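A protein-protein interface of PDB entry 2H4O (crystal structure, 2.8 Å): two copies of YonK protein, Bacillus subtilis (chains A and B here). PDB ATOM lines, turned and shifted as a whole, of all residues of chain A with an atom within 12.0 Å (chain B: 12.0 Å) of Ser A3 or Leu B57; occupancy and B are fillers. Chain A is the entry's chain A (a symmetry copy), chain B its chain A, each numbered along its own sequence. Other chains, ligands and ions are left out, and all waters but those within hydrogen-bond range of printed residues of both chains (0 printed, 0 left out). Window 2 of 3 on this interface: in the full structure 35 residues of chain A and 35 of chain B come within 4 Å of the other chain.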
ATOM      1  N   ALA A   2      29.458 -15.196  -9.593  1.00  0.00           N
ATOM      2  CA  ALA A   2      28.363 -14.388 -10.220  1.00  0.00           C
ATOM      3  C   ALA A   2      26.988 -15.029 -10.032  1.00  0.00           C
ATOM      4  O   ALA A   2      25.941 -14.415 -10.265  1.00  0.00           O
ATOM      5  CB  ALA A   2      28.646 -14.208 -11.707  1.00  0.00           C
ATOM      6  N   SER A   3      26.995 -16.291  -9.637  1.00  0.00           N
ATOM      7  CA  SER A   3      25.762 -17.001  -9.409  1.00  0.00           C
ATOM      8  C   SER A   3      25.055 -16.337  -8.225  1.00  0.00           C
ATOM      9  O   SER A   3      25.686 -15.989  -7.240  1.00  0.00           O
ATOM     10  CB  SER A   3      26.089 -18.452  -9.099  1.00  0.00           C
ATOM     11  OG  SER A   3      27.054 -18.910 -10.029  1.00  0.00           O
ATOM     12  N   LYS A   4      23.745 -16.162  -8.327  1.00  0.00           N
ATOM     13  CA  LYS A   4      23.009 -15.543  -7.263  1.00  0.00           C
ATOM     14  C   LYS A   4      21.523 -15.779  -7.376  1.00  0.00           C
ATOM     15  O   LYS A   4      21.014 -16.192  -8.410  1.00  0.00           O
ATOM     16  CB  LYS A   4      23.283 -14.048  -7.279  1.00  0.00           C
ATOM     17  CG  LYS A   4      23.016 -13.391  -8.593  1.00  0.00           C
ATOM     18  CD  LYS A   4      23.042 -11.888  -8.454  1.00  0.00           C
ATOM     19  CE  LYS A   4      23.155 -11.222  -9.831  1.00  0.00           C
ATOM     20  NZ  LYS A   4      22.722  -9.789  -9.852  1.00  0.00           N
ATOM     21  N   LYS A   5      20.837 -15.496  -6.279  1.00  0.00           N
ATOM     22  CA  LYS A   5      19.389 -15.597  -6.184  1.00  0.00           C
ATOM     23  C   LYS A   5      18.873 -14.144  -6.121  1.00  0.00           C
ATOM     24  O   LYS A   5      19.262 -13.370  -5.273  1.00  0.00           O
ATOM     25  CB  LYS A   5      19.009 -16.339  -4.899  1.00  0.00           C
ATOM     26  CG  LYS A   5      17.511 -16.480  -4.659  1.00  0.00           C
ATOM     27  CD  LYS A   5      17.188 -16.855  -3.215  1.00  0.00           C
ATOM     28  CE  LYS A   5      17.974 -18.068  -2.758  1.00  0.00           C
ATOM     29  NZ  LYS A   5      18.001 -18.181  -1.258  1.00  0.00           N
ATOM     30  N   VAL A   6      18.016 -13.761  -7.040  1.00  0.00           N
ATOM     31  CA  VAL A   6      17.482 -12.423  -7.006  1.00  0.00           C
ATOM     32  C   VAL A   6      15.987 -12.487  -6.670  1.00  0.00           C
ATOM     33  O   VAL A   6      15.300 -13.424  -7.043  1.00  0.00           O
ATOM     34  CB  VAL A   6      17.727 -11.715  -8.335  1.00  0.00           C
ATOM     35  CG2 VAL A   6      16.882 -10.516  -8.414  1.00  0.00           C
ATOM     36  N   HIS A   7      15.504 -11.519  -5.901  1.00  0.00           N
ATOM     37  CA  HIS A   7      14.094 -11.441  -5.534  1.00  0.00           C
ATOM     38  C   HIS A   7      13.742  -9.980  -5.739  1.00  0.00           C
ATOM     39  O   HIS A   7      14.301  -9.114  -5.098  1.00  0.00           O
ATOM     40  CB  HIS A   7      13.884 -11.824  -4.079  1.00  0.00           C
ATOM     41  CG  HIS A   7      12.521 -11.481  -3.562  1.00  0.00           C
ATOM     42  ND1 HIS A   7      11.363 -11.810  -4.233  1.00  0.00           N
ATOM     43  CD2 HIS A   7      12.127 -10.829  -2.439  1.00  0.00           C
ATOM     44  CE1 HIS A   7      10.312 -11.376  -3.553  1.00  0.00           C
ATOM     45  NE2 HIS A   7      10.751 -10.778  -2.460  1.00  0.00           N
ATOM     46  N   LYS B  52      14.742  -4.599  -5.026  1.00  0.00           N
ATOM     47  CA  LYS B  52      15.439  -5.818  -5.394  1.00  0.00           C
ATOM     48  C   LYS B  52      16.301  -6.184  -4.220  1.00  0.00           C
ATOM     49  O   LYS B  52      16.783  -5.308  -3.512  1.00  0.00           O
ATOM     50  CB  LYS B  52      16.314  -5.552  -6.663  1.00  0.00           C
ATOM     51  CG  LYS B  52      17.009  -6.750  -7.281  1.00  0.00           C
ATOM     52  CD  LYS B  52      18.414  -6.441  -7.719  1.00  0.00           C
ATOM     53  CE  LYS B  52      18.471  -5.550  -8.932  1.00  0.00           C
ATOM     54  NZ  LYS B  52      19.869  -5.071  -9.234  1.00  0.00           N
ATOM     55  N   GLU B  53      16.461  -7.482  -4.017  1.00  0.00           N
ATOM     56  CA  GLU B  53      17.273  -8.025  -2.958  1.00  0.00           C
ATOM     57  C   GLU B  53      17.952  -9.232  -3.552  1.00  0.00           C
ATOM     58  O   GLU B  53      17.281 -10.172  -3.916  1.00  0.00           O
ATOM     59  CB  GLU B  53      16.415  -8.485  -1.806  1.00  0.00           C
ATOM     60  CG  GLU B  53      17.234  -9.254  -0.777  1.00  0.00           C
ATOM     61  CD  GLU B  53      16.399 -10.168   0.115  1.00  0.00           C
ATOM     62  OE1 GLU B  53      16.989 -10.804   1.020  1.00  0.00           O
ATOM     63  OE2 GLU B  53      15.160 -10.263  -0.090  1.00  0.00           O
ATOM     64  N   GLU B  54      19.271  -9.226  -3.673  1.00  0.00           N
ATOM     65  CA  GLU B  54      19.945 -10.384  -4.228  1.00  0.00           C
ATOM     66  C   GLU B  54      20.917 -11.049  -3.238  1.00  0.00           C
ATOM     67  O   GLU B  54      21.691 -10.387  -2.593  1.00  0.00           O
ATOM     68  CB  GLU B  54      20.632  -9.991  -5.539  1.00  0.00           C
ATOM     69  CG  GLU B  54      21.434  -8.714  -5.508  1.00  0.00           C
ATOM     70  CD  GLU B  54      22.258  -8.500  -6.774  1.00  0.00           C
ATOM     71  OE1 GLU B  54      21.657  -8.144  -7.816  1.00  0.00           O
ATOM     72  OE2 GLU B  54      23.505  -8.708  -6.711  1.00  0.00           O
ATOM     73  N   ASN B  55      20.859 -12.362  -3.103  1.00  0.00           N
ATOM     74  CA  ASN B  55      21.729 -13.064  -2.177  1.00  0.00           C
ATOM     75  C   ASN B  55      22.586 -14.058  -2.917  1.00  0.00           C
ATOM     76  O   ASN B  55      22.563 -14.110  -4.139  1.00  0.00           O
ATOM     77  CB  ASN B  55      20.891 -13.800  -1.162  1.00  0.00           C
ATOM     78  CG  ASN B  55      19.739 -12.958  -0.656  1.00  0.00           C
ATOM     79  OD1 ASN B  55      19.952 -11.953   0.026  1.00  0.00           O
ATOM     80  ND2 ASN B  55      18.508 -13.349  -1.001  1.00  0.00           N
ATOM     81  N   GLU B  56      23.332 -14.865  -2.170  1.00  0.00           N
ATOM     82  CA  GLU B  56      24.230 -15.867  -2.752  1.00  0.00           C
ATOM     83  C   GLU B  56      23.528 -17.204  -2.886  1.00  0.00           C
ATOM     84  O   GLU B  56      22.526 -17.466  -2.215  1.00  0.00           O
ATOM     85  CB  GLU B  56      25.437 -16.054  -1.862  1.00  0.00           C
ATOM     86  CG  GLU B  56      26.330 -14.863  -1.755  1.00  0.00           C
ATOM     87  CD  GLU B  56      27.213 -14.738  -2.966  1.00  0.00           C
ATOM     88  OE1 GLU B  56      28.187 -13.933  -2.938  1.00  0.00           O
ATOM     89  OE2 GLU B  56      26.925 -15.468  -3.951  1.00  0.00           O
ATOM     90  N   LEU B  57      24.057 -18.060  -3.744  1.00  0.00           N
ATOM     91  CA  LEU B  57      23.444 -19.359  -3.941  1.00  0.00           C
ATOM     92  C   LEU B  57      23.992 -20.376  -2.965  1.00  0.00           C
ATOM     93  O   LEU B  57      25.212 -20.500  -2.815  1.00  0.00           O
ATOM     94  CB  LEU B  57      23.705 -19.887  -5.356  1.00  0.00           C
ATOM     95  CG  LEU B  57      22.867 -19.395  -6.518  1.00  0.00           C
ATOM     96  CD1 LEU B  57      23.179 -20.233  -7.750  1.00  0.00           C
ATOM     97  CD2 LEU B  57      21.411 -19.499  -6.149  1.00  0.00           C
ATOM     98  N   PRO B  58      23.097 -21.135  -2.295  1.00  0.00           N
ATOM     99  CA  PRO B  58      23.534 -22.158  -1.345  1.00  0.00           C
ATOM    100  C   PRO B  58      24.420 -23.179  -2.098  1.00  0.00           C
ATOM    101  O   PRO B  58      23.984 -23.803  -3.072  1.00  0.00           O
ATOM    102  CB  PRO B  58      22.209 -22.746  -0.858  1.00  0.00           C
ATOM    103  CG  PRO B  58      21.319 -22.593  -2.032  1.00  0.00           C
ATOM    104  CD  PRO B  58      21.632 -21.181  -2.460  1.00  0.00           C
ATOM    105  N   VAL B  59      25.668 -23.311  -1.662  1.00  0.00           N
ATOM    106  CA  VAL B  59      26.611 -24.235  -2.280  1.00  0.00           C
ATOM    107  C   VAL B  59      26.434 -25.650  -1.741  1.00  0.00           C
ATOM    108  O   VAL B  59      25.557 -25.928  -0.918  1.00  0.00           O
ATOM    109  CB  VAL B  59      28.050 -23.830  -1.977  1.00  0.00           C
ATOM    110  CG1 VAL B  59      28.466 -22.680  -2.858  1.00  0.00           C
ATOM    111  CG2 VAL B  59      28.157 -23.426  -0.509  1.00  0.00           C
ATOM    112  N   LYS B  60      27.265 -26.556  -2.224  1.00  0.00           N
ATOM    113  CA  LYS B  60      27.213 -27.910  -1.736  1.00  0.00           C
ATOM    114  C   LYS B  60      28.658 -28.398  -1.706  1.00  0.00           C
ATOM    115  O   LYS B  60      28.933 -29.513  -1.261  1.00  0.00           O
ATOM    116  CB  LYS B  60      26.345 -28.787  -2.644  1.00  0.00           C
ATOM    117  CG  LYS B  60      27.000 -29.179  -3.954  1.00  0.00           C
ATOM    118  CD  LYS B  60      26.163 -30.211  -4.700  1.00  0.00           C
ATOM    119  CE  LYS B  60      26.046 -31.519  -3.926  1.00  0.00           C
ATOM    120  NZ  LYS B  60      25.305 -32.542  -4.700  1.00  0.00           N
ATOM    121  N   GLY B  61      29.574 -27.543  -2.168  1.00  0.00           N
ATOM    122  CA  GLY B  61      30.983 -27.899  -2.193  1.00  0.00           C
ATOM    123  C   GLY B  61      31.971 -26.756  -2.406  1.00  0.00           C
ATOM    124  O   GLY B  61      32.367 -26.436  -3.540  1.00  0.00           O
ATOM    125  N   VAL B  62      32.379 -26.125  -1.310  1.00  0.00           N
ATOM    126  CA  VAL B  62      33.341 -25.032  -1.394  1.00  0.00           C
ATOM    127  C   VAL B  62      34.708 -25.711  -1.446  1.00  0.00           C
ATOM    128  O   VAL B  62      34.885 -26.785  -0.855  1.00  0.00           O
ATOM    129  CB  VAL B  62      33.294 -24.099  -0.140  1.00  0.00           C
ATOM    130  CG1 VAL B  62      34.205 -22.900  -0.365  1.00  0.00           C
ATOM    131  CG2 VAL B  62      31.869 -23.634   0.147  1.00  0.00           C
ATOM    132  N   GLU B  63      35.659 -25.096  -2.152  1.00  0.00           N
ATOM    133  CA  GLU B  63      37.018 -25.644  -2.291  1.00  0.00           C
ATOM    134  C   GLU B  63      37.998 -24.630  -2.856  1.00  0.00           C
ATOM    135  O   GLU B  63      37.615 -23.535  -3.283  1.00  0.00           O
ATOM    136  CB  GLU B  63      37.048 -26.842  -3.238  1.00  0.00           C
ATOM    137  CG  GLU B  63      36.497 -28.143  -2.712  1.00  0.00           C
ATOM    138  CD  GLU B  63      36.778 -29.248  -3.684  1.00  0.00           C
ATOM    139  OE1 GLU B  63      36.333 -30.389  -3.432  1.00  0.00           O
ATOM    140  OE2 GLU B  63      37.453 -28.954  -4.704  1.00  0.00           O
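The side-chain carboxylate of Glu B54 lies within salt-bridge range of the side-chain amino group of Lys A4 (2.8 Å). The backbone carbonyl oxygen (O) of Lys A5 lies within hydrogen-bond range of the backbone NH (N) of Asn B55 (2.9 Å). O of His A7 lies within hydrogen-bond range of N of Glu B53.
OD1 of Asn B55 sits close to OE1 of Glu B53 (3.3 Å). The side-chain carboxylate (OE1) of Glu B54 lies within salt-bridge range of the side-chain amino group (NZ) of Lys B52 (3.8 Å).
Glu B56 touches Ser A3 (OE2 to O, 3.6 Å). CB of Ser A3 touches CD1 of Leu B57 (3.7 Å). Lys A4 touches Asn B55 (CB to O, 3.2 Å). Lys A4 touches Leu B57. O of Lys A5 touches O of Glu B53, 3.999 Å away. O of Lys A5 touches CA of Glu B54, 3.2 Å away. Val A6 touches Lys B52. Val A6 touches Glu B53 (C to O, 3.8 Å). Lys B52 touches His A7.
No residue of chain B comes within 4 Å of Ala A2. Printed residues of chain B within 4 Å of Lys A5: Glu B53, Glu B54 and Asn B55. Of the printed residues of chain A, Glu B53 touches Lys A5 (3.999 Å), Val A6 (3.8 Å) and His A7 (2.9 Å). Of the printed residues of chain A, Asn B55 touches Lys A4 (3.2 Å) and Lys A5 (2.9 Å). Of chain A, only Ser A3 comes within 4 Å of Glu B56. Of chain A, only Ser A3 and Lys A4 come within 4 Å of Leu B57. No residue of chain A comes within 4 Å of Pro B58. No residue of chain A comes within 4 Å of Val B59. Gly B61 touches none of the printed residues of chain A. Val B62 touches none of the printed residues of chain A. The nearest residue of chain A that does not touch Leu B57 is Lys A5 (4.05 Å). The nearest printed residue of chain B that does not touch His A7 is Glu B54 (4.9 Å).
Hydrophobic or aromatic side chains of chain B within 4 Å of the printed part of chain A: Leu B57. Of the 6 printed residues of chain A, 5 touch a printed residue of chain B. Hydrophobic or aromatic side chains of chain A that line the printed part of chain B: Val A6 and His A7. Along chain A the printed residues that touch a printed residue of chain B span positions 3 to 7. Among the printed residues, 12 pairs touch across the chains. Among the printed residues, Asp or Glu carboxylates within 4 Å of a Lys or Arg side-chain nitrogen of the other chain: Lys A4 with Glu B54.
No position is printed for both chains. Of the 12 pairs that touch across the chains among the printed residues, none has its exchanged pair printed and touching as well.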
